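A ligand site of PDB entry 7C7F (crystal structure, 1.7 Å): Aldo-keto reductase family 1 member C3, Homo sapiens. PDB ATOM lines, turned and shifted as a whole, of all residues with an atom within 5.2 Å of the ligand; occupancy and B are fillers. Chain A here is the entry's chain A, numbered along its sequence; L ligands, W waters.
The guanidinium group of Arg 278 is in salt-bridge range of an oxygen (O17) of the ligand. OE1 of Gln 281 lies within hydrogen-bond range of N3 of the ligand (2.6 Å). An oxygen (O8) of the ligand lies within hydrogen-bond range of the side-chain amide nitrogen (NE2) of Gln 224, at 2.7 Å. The side-chain hydroxyl of Ser 273 sits at hydrogen-bond distance from an oxygen (O17) of the ligand (2.7 Å). The backbone NH (N) of Lys 272 is in hydrogen-bond range of an oxygen (O1) of the ligand. An oxygen (O15) of the ligand lies within salt-bridge range of the side-chain amino group (NZ) of Lys 272 (2.7 Å). OG of Ser 168 lies within hydrogen-bond range of N7 of the ligand (2.7 Å). O13 of the ligand lies within hydrogen-bond range of OD2 of Asp 52, 2.7 Å away. The backbone NH of Ser 219 lies within hydrogen-bond range of an oxygen (O10) of the ligand (3.2 Å). OG of Ser 219 sits at hydrogen-bond distance from O9 of the ligand (2.8 Å). The backbone NH (N) of Tyr 274 lies within hydrogen-bond range of an oxygen (O15) of the ligand (2.9 Å). The side-chain amide oxygen (OD1) of Asn 282 sits at hydrogen-bond distance from a nitrogen (N3) of the ligand (2.9 Å). The side-chain amide oxygen of Gln 192 is in hydrogen-bond range of a nitrogen (N7) of the ligand, at 3.0 Å. An oxygen (O14) of the ligand sits at hydrogen-bond distance from the side-chain amide nitrogen (ND2) of Asn 169. N of Ser 223 is in hydrogen-bond range of O2 of the ligand (3.0 Å). O2 of the ligand sits at hydrogen-bond distance from N of Leu 221 (3.1 Å). The backbone NH (N) of Tyr 26 sits at hydrogen-bond distance from an oxygen (O12) of the ligand (3.2 Å). The backbone NH (N) of Gly 222 lies within hydrogen-bond range of an oxygen (O2) of the ligand (3.3 Å).
The backbone carbonyl oxygen of Arg 278 lies close to the side-chain amide nitrogen of Asn 282. The side-chain hydroxyl (OG1) of Thr 253 is in hydrogen-bond range of the side-chain amide oxygen (OE1) of Gln 281, 2.6 Å away. The backbone carbonyl oxygen (O) of Tyr 26 lies within hydrogen-bond range of the side-chain amide nitrogen (NE2) of Gln 224 (2.9 Å). The side-chain hydroxyl (OG) of Ser 168 lies close to the backbone carbonyl oxygen (O) of His 119, 3.4 Å away. The side-chain carboxylate (OD1) of Asp 52 is in hydrogen-bond range of the side-chain amide nitrogen (NE2) of Gln 192, at 2.9 Å. OH of Tyr 218 is in hydrogen-bond range of OD1 of Asn 169, at 2.8 Å. ND2 of Asn 169 lies within hydrogen-bond range of O of His 119 (3.0 Å). The side-chain amino group of Lys 86 sits at hydrogen-bond distance from the side-chain hydroxyl of Tyr 57, at 3.1 Å.
The side-chain hydroxyl (OH) of Tyr 57 sits close to a nitrogen (N6) of the ligand, 3.4 Å away. Residues that only touch the ligand: Gly 24 (3.3 Å), Thr 25 (3.6 Å), Lys 86 (3.8 Å), His 119 (3.5 Å), Tyr 218 (3.2 Å), Ala 220 (3.5 Å), Leu 238 (3.5 Å), Ala 255 (3.3 Å), Leu 270 (3.5 Å), Ala 271 (3.5 Å) and Asn 275 (3.9 Å). Hydrophobic or aromatic side chains that line the ligand: Tyr 26, Tyr 57, His 119, Tyr 218, Leu 221, Leu 238, Ala 255 and Leu 270. Of the 32 residues printed, 28 come within 4 Å of the ligand. The nearest printed residue that does not touch the ligand is Phe 308 (4.02 Å).
Water W6 lies within hydrogen-bond range of O of Leu 270 (2.6 Å), O1 of the ligand (2.6 Å), N of Ala 220 (2.8 Å) and N of Ser 219 (3.1 Å). Water W2 lies within hydrogen-bond range of O8 of the ligand (2.7 Å) and NE2 of Gln 224 (3.3 Å). Water W1 lies within hydrogen-bond range of the backbone NH (N) of Ala 255 (2.9 Å), a nitrogen (N4) of the ligand (3.0 Å) and the side-chain hydroxyl (OG1) of Thr 253 (3.3 Å). Water W4 bridges NE2 of Gln 281 and N4 of the ligand.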
ATOM      1  N   PHE A  23     -18.103   4.366  33.493  1.00  0.00           N
ATOM      2  CA  PHE A  23     -19.065   4.248  32.407  1.00  0.00           C
ATOM      3  C   PHE A  23     -18.450   3.560  31.185  1.00  0.00           C
ATOM      4  O   PHE A  23     -17.447   4.040  30.628  1.00  0.00           O
ATOM      5  CB  PHE A  23     -19.585   5.634  32.036  1.00  0.00           C
ATOM      6  CG  PHE A  23     -20.623   5.645  30.922  1.00  0.00           C
ATOM      7  CD1 PHE A  23     -21.849   5.030  31.100  1.00  0.00           C
ATOM      8  CD2 PHE A  23     -20.354   6.285  29.720  1.00  0.00           C
ATOM      9  CE1 PHE A  23     -22.805   5.033  30.085  1.00  0.00           C
ATOM     10  CE2 PHE A  23     -21.328   6.315  28.692  1.00  0.00           C
ATOM     11  CZ  PHE A  23     -22.544   5.682  28.876  1.00  0.00           C
ATOM     12  N   GLY A  24     -19.061   2.464  30.751  1.00  0.00           N
ATOM     13  CA  GLY A  24     -18.607   1.780  29.543  1.00  0.00           C
ATOM     14  C   GLY A  24     -19.232   2.398  28.279  1.00  0.00           C
ATOM     15  O   GLY A  24     -20.457   2.497  28.172  1.00  0.00           O
ATOM     16  N   THR A  25     -18.387   2.766  27.323  1.00  0.00           N
ATOM     17  CA  THR A  25     -18.851   3.504  26.139  1.00  0.00           C
ATOM     18  C   THR A  25     -18.998   2.645  24.883  1.00  0.00           C
ATOM     19  O   THR A  25     -19.421   3.174  23.860  1.00  0.00           O
ATOM     20  CB  THR A  25     -17.916   4.679  25.830  1.00  0.00           C
ATOM     21  OG1 THR A  25     -16.622   4.201  25.385  1.00  0.00           O
ATOM     22  CG2 THR A  25     -17.780   5.608  27.053  1.00  0.00           C
ATOM     23  N   TYR A  26     -18.626   1.348  24.920  1.00  0.00           N
ATOM     24  CA  TYR A  26     -18.663   0.565  23.694  1.00  0.00           C
ATOM     25  C   TYR A  26     -20.100   0.339  23.232  1.00  0.00           C
ATOM     26  O   TYR A  26     -20.960  -0.053  24.022  1.00  0.00           O
ATOM     27  CB  TYR A  26     -17.990  -0.808  23.865  1.00  0.00           C
ATOM     28  CG  TYR A  26     -18.093  -1.543  22.539  1.00  0.00           C
ATOM     29  CD1 TYR A  26     -17.369  -1.095  21.440  1.00  0.00           C
ATOM     30  CD2 TYR A  26     -18.962  -2.621  22.355  1.00  0.00           C
ATOM     31  CE1 TYR A  26     -17.467  -1.701  20.196  1.00  0.00           C
ATOM     32  CE2 TYR A  26     -19.080  -3.243  21.096  1.00  0.00           C
ATOM     33  CZ  TYR A  26     -18.321  -2.775  20.029  1.00  0.00           C
ATOM     34  OH  TYR A  26     -18.395  -3.345  18.769  1.00  0.00           O
ATOM     35  N   ASP A  52     -14.817   4.944  30.228  1.00  0.00           N
ATOM     36  CA  ASP A  52     -13.961   3.965  29.568  1.00  0.00           C
ATOM     37  C   ASP A  52     -14.191   3.873  28.070  1.00  0.00           C
ATOM     38  O   ASP A  52     -15.280   3.542  27.617  1.00  0.00           O
ATOM     39  CB  ASP A  52     -14.177   2.585  30.207  1.00  0.00           C
ATOM     40  CG  ASP A  52     -13.197   1.547  29.701  1.00  0.00           C
ATOM     41  OD1 ASP A  52     -12.071   1.486  30.228  1.00  0.00           O
ATOM     42  OD2 ASP A  52     -13.550   0.775  28.789  1.00  0.00           O
ATOM     43  N   SER A  53     -13.123   4.113  27.324  1.00  0.00           N
ATOM     44  CA  SER A  53     -13.149   4.079  25.865  1.00  0.00           C
ATOM     45  C   SER A  53     -11.886   3.429  25.333  1.00  0.00           C
ATOM     46  O   SER A  53     -11.026   3.029  26.097  1.00  0.00           O
ATOM     47  CB  SER A  53     -13.322   5.469  25.267  1.00  0.00           C
ATOM     48  OG  SER A  53     -13.448   5.390  23.862  1.00  0.00           O
ATOM     49  N   TYR A  57     -13.107   1.185  19.780  1.00  0.00           N
ATOM     50  CA  TYR A  57     -14.533   1.469  19.895  1.00  0.00           C
ATOM     51  C   TYR A  57     -15.037   2.467  18.862  1.00  0.00           C
ATOM     52  O   TYR A  57     -16.264   2.681  18.785  1.00  0.00           O
ATOM     53  CB  TYR A  57     -14.862   1.984  21.301  1.00  0.00           C
ATOM     54  CG  TYR A  57     -14.501   1.024  22.429  1.00  0.00           C
ATOM     55  CD1 TYR A  57     -14.146  -0.310  22.161  1.00  0.00           C
ATOM     56  CD2 TYR A  57     -14.527   1.436  23.744  1.00  0.00           C
ATOM     57  CE1 TYR A  57     -13.792  -1.180  23.224  1.00  0.00           C
ATOM     58  CE2 TYR A  57     -14.183   0.577  24.790  1.00  0.00           C
ATOM     59  CZ  TYR A  57     -13.832  -0.726  24.526  1.00  0.00           C
ATOM     60  OH  TYR A  57     -13.505  -1.533  25.603  1.00  0.00           O
ATOM     61  N   LYS A  86      -7.277   3.001  25.289  1.00  0.00           N
ATOM     62  CA  LYS A  86      -6.597   1.711  25.208  1.00  0.00           C
ATOM     63  C   LYS A  86      -5.808   1.664  23.911  1.00  0.00           C
ATOM     64  O   LYS A  86      -6.243   2.189  22.882  1.00  0.00           O
ATOM     65  CB  LYS A  86      -7.578   0.543  25.301  1.00  0.00           C
ATOM     66  CG  LYS A  86      -8.531   0.584  26.507  1.00  0.00           C
ATOM     67  CD  LYS A  86      -9.206  -0.770  26.681  1.00  0.00           C
ATOM     68  CE  LYS A  86     -10.320  -0.724  27.751  1.00  0.00           C
ATOM     69  NZ  LYS A  86     -11.519   0.069  27.295  1.00  0.00           N
ATOM     70  N   HIS A 119      -4.616  -2.802  25.469  1.00  0.00           N
ATOM     71  CA  HIS A 119      -5.977  -3.337  25.382  1.00  0.00           C
ATOM     72  C   HIS A 119      -5.980  -4.848  25.586  1.00  0.00           C
ATOM     73  O   HIS A 119      -6.865  -5.363  26.279  1.00  0.00           O
ATOM     74  CB  HIS A 119      -6.591  -2.982  24.020  1.00  0.00           C
ATOM     75  CG  HIS A 119      -8.095  -2.984  24.012  1.00  0.00           C
ATOM     76  ND1 HIS A 119      -8.819  -2.256  23.099  1.00  0.00           N
ATOM     77  CD2 HIS A 119      -8.996  -3.625  24.786  1.00  0.00           C
ATOM     78  CE1 HIS A 119     -10.111  -2.449  23.311  1.00  0.00           C
ATOM     79  NE2 HIS A 119     -10.248  -3.269  24.337  1.00  0.00           N
ATOM     80  N   SER A 168      -4.930  -4.588  30.357  1.00  0.00           N
ATOM     81  CA  SER A 168      -6.257  -5.158  30.245  1.00  0.00           C
ATOM     82  C   SER A 168      -6.135  -6.553  29.650  1.00  0.00           C
ATOM     83  O   SER A 168      -5.367  -6.758  28.708  1.00  0.00           O
ATOM     84  CB  SER A 168      -7.198  -4.331  29.361  1.00  0.00           C
ATOM     85  OG  SER A 168      -8.474  -4.946  29.302  1.00  0.00           O
ATOM     86  N   ASN A 169      -6.921  -7.492  30.191  1.00  0.00           N
ATOM     87  CA  ASN A 169      -6.963  -8.883  29.749  1.00  0.00           C
ATOM     88  C   ASN A 169      -5.653  -9.621  29.980  1.00  0.00           C
ATOM     89  O   ASN A 169      -5.343 -10.556  29.249  1.00  0.00           O
ATOM     90  CB  ASN A 169      -7.347  -9.003  28.271  1.00  0.00           C
ATOM     91  CG  ASN A 169      -8.734  -8.444  27.989  1.00  0.00           C
ATOM     92  OD1 ASN A 169      -9.704  -8.850  28.625  1.00  0.00           O
ATOM     93  ND2 ASN A 169      -8.827  -7.525  27.020  1.00  0.00           N
ATOM     94  N   GLN A 192      -7.670  -4.431  33.850  1.00  0.00           N
ATOM     95  CA  GLN A 192      -9.089  -4.432  33.515  1.00  0.00           C
ATOM     96  C   GLN A 192      -9.430  -5.718  32.772  1.00  0.00           C
ATOM     97  O   GLN A 192      -8.889  -5.969  31.694  1.00  0.00           O
ATOM     98  CB  GLN A 192      -9.455  -3.212  32.653  1.00  0.00           C
ATOM     99  CG  GLN A 192     -10.923  -3.261  32.194  1.00  0.00           C
ATOM    100  CD  GLN A 192     -11.314  -2.174  31.182  1.00  0.00           C
ATOM    101  OE1 GLN A 192     -11.875  -2.476  30.112  1.00  0.00           O
ATOM    102  NE2 GLN A 192     -11.050  -0.917  31.515  1.00  0.00           N
ATOM    103  N   TYR A 218     -14.977  -5.452  33.619  1.00  0.00           N
ATOM    104  CA  TYR A 218     -15.861  -5.202  32.491  1.00  0.00           C
ATOM    105  C   TYR A 218     -16.816  -6.376  32.320  1.00  0.00           C
ATOM    106  O   TYR A 218     -16.649  -7.426  32.935  1.00  0.00           O
ATOM    107  CB  TYR A 218     -15.062  -4.923  31.204  1.00  0.00           C
ATOM    108  CG  TYR A 218     -14.386  -6.075  30.467  1.00  0.00           C
ATOM    109  CD1 TYR A 218     -15.119  -7.078  29.828  1.00  0.00           C
ATOM    110  CD2 TYR A 218     -12.997  -6.121  30.362  1.00  0.00           C
ATOM    111  CE1 TYR A 218     -14.492  -8.083  29.140  1.00  0.00           C
ATOM    112  CE2 TYR A 218     -12.366  -7.127  29.684  1.00  0.00           C
ATOM    113  CZ  TYR A 218     -13.105  -8.104  29.070  1.00  0.00           C
ATOM    114  OH  TYR A 218     -12.439  -9.071  28.382  1.00  0.00           O
ATOM    115  N   SER A 219     -17.827  -6.168  31.467  1.00  0.00           N
ATOM    116  CA  SER A 219     -18.956  -7.078  31.323  1.00  0.00           C
ATOM    117  C   SER A 219     -19.543  -7.458  32.677  1.00  0.00           C
ATOM    118  O   SER A 219     -19.988  -8.605  32.882  1.00  0.00           O
ATOM    119  CB  SER A 219     -18.577  -8.324  30.523  1.00  0.00           C
ATOM    120  OG  SER A 219     -18.545  -8.038  29.143  1.00  0.00           O
ATOM    121  N   ALA A 220     -19.498  -6.517  33.625  1.00  0.00           N
ATOM    122  CA  ALA A 220     -19.918  -6.760  34.994  1.00  0.00           C
ATOM    123  C   ALA A 220     -21.418  -6.914  35.123  1.00  0.00           C
ATOM    124  O   ALA A 220     -21.885  -7.372  36.174  1.00  0.00           O
ATOM    125  CB  ALA A 220     -19.439  -5.627  35.891  1.00  0.00           C
ATOM    126  N   LEU A 221     -22.170  -6.518  34.098  1.00  0.00           N
ATOM    127  CA  LEU A 221     -23.598  -6.739  33.974  1.00  0.00           C
ATOM    128  C   LEU A 221     -23.897  -7.912  33.064  1.00  0.00           C
ATOM    129  O   LEU A 221     -25.068  -8.213  32.812  1.00  0.00           O
ATOM    130  CB  LEU A 221     -24.292  -5.464  33.463  1.00  0.00           C
ATOM    131  CG  LEU A 221     -24.138  -4.262  34.404  1.00  0.00           C
ATOM    132  CD1 LEU A 221     -25.094  -3.114  34.039  1.00  0.00           C
ATOM    133  CD2 LEU A 221     -24.325  -4.656  35.861  1.00  0.00           C
ATOM    134  N   GLY A 222     -22.863  -8.571  32.569  1.00  0.00           N
ATOM    135  CA  GLY A 222     -23.038  -9.774  31.784  1.00  0.00           C
ATOM    136  C   GLY A 222     -22.919  -9.635  30.288  1.00  0.00           C
ATOM    137  O   GLY A 222     -23.400 -10.533  29.581  1.00  0.00           O
ATOM    138  N   SER A 223     -22.233  -8.578  29.770  1.00  0.00           N
ATOM    139  CA  SER A 223     -21.891  -8.558  28.346  1.00  0.00           C
ATOM    140  C   SER A 223     -23.147  -7.986  27.680  1.00  0.00           C
ATOM    141  O   SER A 223     -24.209  -7.986  28.315  1.00  0.00           O
ATOM    142  CB  SER A 223     -21.176  -9.830  27.915  1.00  0.00           C
ATOM    143  OG  SER A 223     -22.141 -10.675  27.316  1.00  0.00           O
ATOM    144  N   GLN A 224     -23.058  -7.426  26.482  1.00  0.00           N
ATOM    145  CA  GLN A 224     -24.202  -6.881  25.754  1.00  0.00           C
ATOM    146  C   GLN A 224     -24.640  -8.050  24.851  1.00  0.00           C
ATOM    147  O   GLN A 224     -25.629  -7.918  24.133  1.00  0.00           O
ATOM    148  CB  GLN A 224     -23.718  -5.742  24.834  1.00  0.00           C
ATOM    149  CG  GLN A 224     -22.987  -4.615  25.558  1.00  0.00           C
ATOM    150  CD  GLN A 224     -22.621  -3.449  24.638  1.00  0.00           C
ATOM    151  OE1 GLN A 224     -23.301  -3.175  23.643  1.00  0.00           O
ATOM    152  NE2 GLN A 224     -21.534  -2.771  24.980  1.00  0.00           N
ATOM    153  N   LEU A 238     -28.349 -11.135  34.283  1.00  0.00           N
ATOM    154  CA  LEU A 238     -29.323 -10.373  35.030  1.00  0.00           C
ATOM    155  C   LEU A 238     -30.614 -11.143  35.272  1.00  0.00           C
ATOM    156  O   LEU A 238     -31.409 -10.738  36.121  1.00  0.00           O
ATOM    157  CB  LEU A 238     -29.592  -9.045  34.323  1.00  0.00           C
ATOM    158  CG  LEU A 238     -28.316  -8.199  34.347  1.00  0.00           C
ATOM    159  CD1 LEU A 238     -28.600  -6.812  33.840  1.00  0.00           C
ATOM    160  CD2 LEU A 238     -27.741  -8.156  35.753  1.00  0.00           C
ATOM    161  N   THR A 253     -32.243  -3.374  41.688  1.00  0.00           N
ATOM    162  CA  THR A 253     -32.350  -4.170  40.475  1.00  0.00           C
ATOM    163  C   THR A 253     -31.207  -5.176  40.436  1.00  0.00           C
ATOM    164  O   THR A 253     -30.218  -5.030  41.164  1.00  0.00           O
ATOM    165  CB  THR A 253     -32.282  -3.275  39.236  1.00  0.00           C
ATOM    166  OG1 THR A 253     -30.979  -2.682  39.156  1.00  0.00           O
ATOM    167  CG2 THR A 253     -33.334  -2.179  39.303  1.00  0.00           C
ATOM    168  N   ALA A 255     -28.943  -5.576  38.205  1.00  0.00           N
ATOM    169  CA  ALA A 255     -27.743  -4.826  37.824  1.00  0.00           C
ATOM    170  C   ALA A 255     -27.115  -4.144  39.026  1.00  0.00           C
ATOM    171  O   ALA A 255     -25.886  -4.204  39.210  1.00  0.00           O
ATOM    172  CB  ALA A 255     -28.094  -3.785  36.752  1.00  0.00           C
ATOM    173  N   LEU A 270     -17.159  -1.252  35.846  1.00  0.00           N
ATOM    174  CA  LEU A 270     -17.712  -0.549  34.691  1.00  0.00           C
ATOM    175  C   LEU A 270     -19.138  -0.986  34.442  1.00  0.00           C
ATOM    176  O   LEU A 270     -19.532  -2.108  34.780  1.00  0.00           O
ATOM    177  CB  LEU A 270     -16.878  -0.820  33.435  1.00  0.00           C
ATOM    178  CG  LEU A 270     -15.381  -0.544  33.497  1.00  0.00           C
ATOM    179  CD1 LEU A 270     -14.728  -0.808  32.157  1.00  0.00           C
ATOM    180  CD2 LEU A 270     -15.066   0.838  34.014  1.00  0.00           C
ATOM    181  N   ALA A 271     -19.933  -0.076  33.865  1.00  0.00           N
ATOM    182  CA  ALA A 271     -21.297  -0.375  33.478  1.00  0.00           C
ATOM    183  C   ALA A 271     -21.579   0.369  32.179  1.00  0.00           C
ATOM    184  O   ALA A 271     -21.476   1.597  32.131  1.00  0.00           O
ATOM    185  CB  ALA A 271     -22.313   0.011  34.562  1.00  0.00           C
ATOM    186  N   LYS A 272     -21.833  -0.392  31.115  1.00  0.00           N
ATOM    187  CA  LYS A 272     -22.284   0.219  29.875  1.00  0.00           C
ATOM    188  C   LYS A 272     -23.792   0.326  29.920  1.00  0.00           C
ATOM    189  O   LYS A 272     -24.472  -0.603  30.330  1.00  0.00           O
ATOM    190  CB  LYS A 272     -21.867  -0.573  28.630  1.00  0.00           C
ATOM    191  CG  LYS A 272     -22.466  -0.042  27.307  1.00  0.00           C
ATOM    192  CD  LYS A 272     -23.776  -0.743  26.924  1.00  0.00           C
ATOM    193  CE  LYS A 272     -24.214  -0.421  25.509  1.00  0.00           C
ATOM    194  NZ  LYS A 272     -25.529  -1.086  25.205  1.00  0.00           N
ATOM    195  N   SER A 273     -24.298   1.480  29.516  1.00  0.00           N
ATOM    196  CA  SER A 273     -25.699   1.570  29.161  1.00  0.00           C
ATOM    197  C   SER A 273     -25.852   2.765  28.233  1.00  0.00           C
ATOM    198  O   SER A 273     -25.214   3.797  28.462  1.00  0.00           O
ATOM    199  CB  SER A 273     -26.605   1.706  30.379  1.00  0.00           C
ATOM    200  OG  SER A 273     -27.941   1.942  29.949  1.00  0.00           O
ATOM    201  N   TYR A 274     -26.643   2.581  27.178  1.00  0.00           N
ATOM    202  CA  TYR A 274     -27.018   3.644  26.254  1.00  0.00           C
ATOM    203  C   TYR A 274     -28.475   4.062  26.454  1.00  0.00           C
ATOM    204  O   TYR A 274     -29.061   4.730  25.583  1.00  0.00           O
ATOM    205  CB  TYR A 274     -26.738   3.191  24.827  1.00  0.00           C
ATOM    206  CG  TYR A 274     -25.337   3.514  24.353  1.00  0.00           C
ATOM    207  CD1 TYR A 274     -25.124   4.035  23.077  1.00  0.00           C
ATOM    208  CD2 TYR A 274     -24.225   3.314  25.172  1.00  0.00           C
ATOM    209  CE1 TYR A 274     -23.848   4.366  22.626  1.00  0.00           C
ATOM    210  CE2 TYR A 274     -22.942   3.612  24.727  1.00  0.00           C
ATOM    211  CZ  TYR A 274     -22.762   4.152  23.453  1.00  0.00           C
ATOM    212  OH  TYR A 274     -21.498   4.457  22.994  1.00  0.00           O
ATOM    213  N   ASN A 275     -29.031   3.722  27.598  1.00  0.00           N
ATOM    214  CA  ASN A 275     -30.397   4.035  27.991  1.00  0.00           C
ATOM    215  C   ASN A 275     -30.387   5.049  29.137  1.00  0.00           C
ATOM    216  O   ASN A 275     -29.827   4.760  30.205  1.00  0.00           O
ATOM    217  CB  ASN A 275     -31.108   2.751  28.427  1.00  0.00           C
ATOM    218  CG  ASN A 275     -32.543   2.990  28.817  1.00  0.00           C
ATOM    219  OD1 ASN A 275     -32.860   3.123  30.010  1.00  0.00           O
ATOM    220  ND2 ASN A 275     -33.431   3.074  27.817  1.00  0.00           N
ATOM    221  N   ARG A 278     -31.424   3.670  32.620  1.00  0.00           N
ATOM    222  CA  ARG A 278     -30.478   2.747  33.250  1.00  0.00           C
ATOM    223  C   ARG A 278     -29.183   3.467  33.619  1.00  0.00           C
ATOM    224  O   ARG A 278     -28.588   3.187  34.664  1.00  0.00           O
ATOM    225  CB  ARG A 278     -30.240   1.544  32.332  1.00  0.00           C
ATOM    226  CG  ARG A 278     -31.463   0.634  32.296  1.00  0.00           C
ATOM    227  CD  ARG A 278     -31.262  -0.633  31.492  1.00  0.00           C
ATOM    228  NE  ARG A 278     -31.317  -0.469  30.037  1.00  0.00           N
ATOM    229  CZ  ARG A 278     -32.437  -0.472  29.312  1.00  0.00           C
ATOM    230  NH1 ARG A 278     -33.618  -0.589  29.895  1.00  0.00           N
ATOM    231  NH2 ARG A 278     -32.378  -0.333  27.997  1.00  0.00           N
ATOM    232  N   GLN A 281     -29.887   4.962  36.791  1.00  0.00           N
ATOM    233  CA  GLN A 281     -30.107   3.985  37.855  1.00  0.00           C
ATOM    234  C   GLN A 281     -28.786   3.421  38.371  1.00  0.00           C
ATOM    235  O   GLN A 281     -28.634   3.167  39.573  1.00  0.00           O
ATOM    236  CB  GLN A 281     -31.016   2.862  37.353  1.00  0.00           C
ATOM    237  CG  GLN A 281     -31.136   1.665  38.301  1.00  0.00           C
ATOM    238  CD  GLN A 281     -31.571   0.405  37.560  1.00  0.00           C
ATOM    239  OE1 GLN A 281     -30.881  -0.614  37.582  1.00  0.00           O
ATOM    240  NE2 GLN A 281     -32.699   0.489  36.876  1.00  0.00           N
ATOM    241  N   ASN A 282     -27.823   3.256  37.482  1.00  0.00           N
ATOM    242  CA  ASN A 282     -26.575   2.592  37.857  1.00  0.00           C
ATOM    243  C   ASN A 282     -25.808   3.377  38.924  1.00  0.00           C
ATOM    244  O   ASN A 282     -25.082   2.778  39.718  1.00  0.00           O
ATOM    245  CB  ASN A 282     -25.755   2.363  36.588  1.00  0.00           C
ATOM    246  CG  ASN A 282     -26.318   1.202  35.750  1.00  0.00           C
ATOM    247  OD1 ASN A 282     -27.100   0.395  36.258  1.00  0.00           O
ATOM    248  ND2 ASN A 282     -25.962   1.149  34.475  1.00  0.00           N
ATOM    249  N   PHE A 308     -17.274 -13.953  26.369  1.00  0.00           N
ATOM    250  CA  PHE A 308     -16.653 -13.771  25.063  1.00  0.00           C
ATOM    251  C   PHE A 308     -15.959 -15.044  24.597  1.00  0.00           C
ATOM    252  O   PHE A 308     -15.187 -15.655  25.332  1.00  0.00           O
ATOM    253  CB  PHE A 308     -15.681 -12.601  25.090  1.00  0.00           C
ATOM    254  CG  PHE A 308     -16.320 -11.310  25.538  1.00  0.00           C
ATOM    255  CD1 PHE A 308     -16.925 -10.474  24.624  1.00  0.00           C
ATOM    256  CD2 PHE A 308     -16.329 -10.962  26.874  1.00  0.00           C
ATOM    257  CE1 PHE A 308     -17.515  -9.298  25.036  1.00  0.00           C
ATOM    258  CE2 PHE A 308     -16.919  -9.787  27.286  1.00  0.00           C
ATOM    259  CZ  PHE A 308     -17.512  -8.955  26.367  1.00  0.00           C
HETATM  260  P1  LIG L   1     -21.968  -4.414  30.622  1.00  0.00           P
HETATM  261  O1  LIG L   1     -21.498  -3.285  31.521  1.00  0.00           O
HETATM  262  O2  LIG L   1     -21.800  -5.861  31.069  1.00  0.00           O
HETATM  263  O3  LIG L   1     -23.549  -4.160  30.374  1.00  0.00           O
HETATM  264  C1  LIG L   1     -24.238  -5.088  29.545  1.00  0.00           C
HETATM  265  C2  LIG L   1     -25.662  -4.615  29.228  1.00  0.00           C
HETATM  266  O4  LIG L   1     -26.403  -4.401  30.425  1.00  0.00           O
HETATM  267  C3  LIG L   1     -25.689  -3.291  28.468  1.00  0.00           C
HETATM  268  O5  LIG L   1     -25.826  -3.545  27.074  1.00  0.00           O
HETATM  269  C4  LIG L   1     -26.912  -2.557  29.003  1.00  0.00           C
HETATM  270  O6  LIG L   1     -27.897  -2.395  27.967  1.00  0.00           O
HETATM  271  C5  LIG L   1     -27.409  -3.427  30.139  1.00  0.00           C
HETATM  272  N1  LIG L   1     -27.647  -2.630  31.365  1.00  0.00           N
HETATM  273  C6  LIG L   1     -26.941  -1.554  31.775  1.00  0.00           C
HETATM  274  N2  LIG L   1     -27.448  -1.085  32.943  1.00  0.00           N
HETATM  275  C7  LIG L   1     -28.517  -1.853  33.267  1.00  0.00           C
HETATM  276  C8  LIG L   1     -29.493  -1.922  34.366  1.00  0.00           C
HETATM  277  N3  LIG L   1     -29.465  -1.039  35.390  1.00  0.00           N
HETATM  278  N4  LIG L   1     -30.424  -2.903  34.328  1.00  0.00           N
HETATM  279  C9  LIG L   1     -30.467  -3.810  33.329  1.00  0.00           C
HETATM  280  N5  LIG L   1     -29.610  -3.809  32.298  1.00  0.00           N
HETATM  281  C10 LIG L   1     -28.634  -2.871  32.221  1.00  0.00           C
HETATM  282  O7  LIG L   1     -21.545  -4.254  29.085  1.00  0.00           O
HETATM  283  P2  LIG L   1     -20.093  -4.372  28.348  1.00  0.00           P
HETATM  284  O8  LIG L   1     -20.135  -3.467  27.147  1.00  0.00           O
HETATM  285  O9  LIG L   1     -19.844  -5.836  28.054  1.00  0.00           O
HETATM  286  O10 LIG L   1     -18.988  -3.953  29.418  1.00  0.00           O
HETATM  287  C11 LIG L   1     -18.892  -2.601  29.891  1.00  0.00           C
HETATM  288  C12 LIG L   1     -17.689  -1.853  29.328  1.00  0.00           C
HETATM  289  O11 LIG L   1     -16.426  -2.473  29.637  1.00  0.00           O
HETATM  290  C13 LIG L   1     -17.679  -1.692  27.819  1.00  0.00           C
HETATM  291  O12 LIG L   1     -18.652  -0.786  27.261  1.00  0.00           O
HETATM  292  C14 LIG L   1     -16.247  -1.247  27.609  1.00  0.00           C
HETATM  293  O13 LIG L   1     -16.115   0.128  28.050  1.00  0.00           O
HETATM  294  C15 LIG L   1     -15.502  -2.160  28.586  1.00  0.00           C
HETATM  295  N6  LIG L   1     -15.046  -3.425  27.969  1.00  0.00           N
HETATM  296  C16 LIG L   1     -13.713  -3.673  27.911  1.00  0.00           C
HETATM  297  C17 LIG L   1     -13.212  -4.840  27.340  1.00  0.00           C
HETATM  298  C18 LIG L   1     -11.727  -5.097  27.270  1.00  0.00           C
HETATM  299  O14 LIG L   1     -11.308  -5.880  26.427  1.00  0.00           O
HETATM  300  N7  LIG L   1     -10.905  -4.498  28.134  1.00  0.00           N
HETATM  301  C19 LIG L   1     -14.098  -5.783  26.833  1.00  0.00           C
HETATM  302  C20 LIG L   1     -15.465  -5.544  26.913  1.00  0.00           C
HETATM  303  C21 LIG L   1     -15.912  -4.344  27.489  1.00  0.00           C
HETATM  304  P3  LIG L   1     -28.514  -0.921  27.657  1.00  0.00           P
HETATM  305  O15 LIG L   1     -27.412  -0.190  26.927  1.00  0.00           O
HETATM  306  O16 LIG L   1     -29.713  -1.202  26.779  1.00  0.00           O
HETATM  307  O17 LIG L   1     -28.902  -0.373  29.002  1.00  0.00           O
HETATM  308  O   HOH W   1     -31.248  -4.765  36.575  1.00  0.00           O
HETATM  309  O   HOH W   2     -18.438  -3.985  25.073  1.00  0.00           O
HETATM  310  O   HOH W   3     -29.585   0.942  24.446  1.00  0.00           O
HETATM  311  O   HOH W   4     -33.367  -1.665  34.959  1.00  0.00           O
HETATM  312  O   HOH W   5     -27.977  -5.141  26.256  1.00  0.00           O
HETATM  313  O   HOH W   6     -19.281  -3.863  32.839  1.00  0.00           O
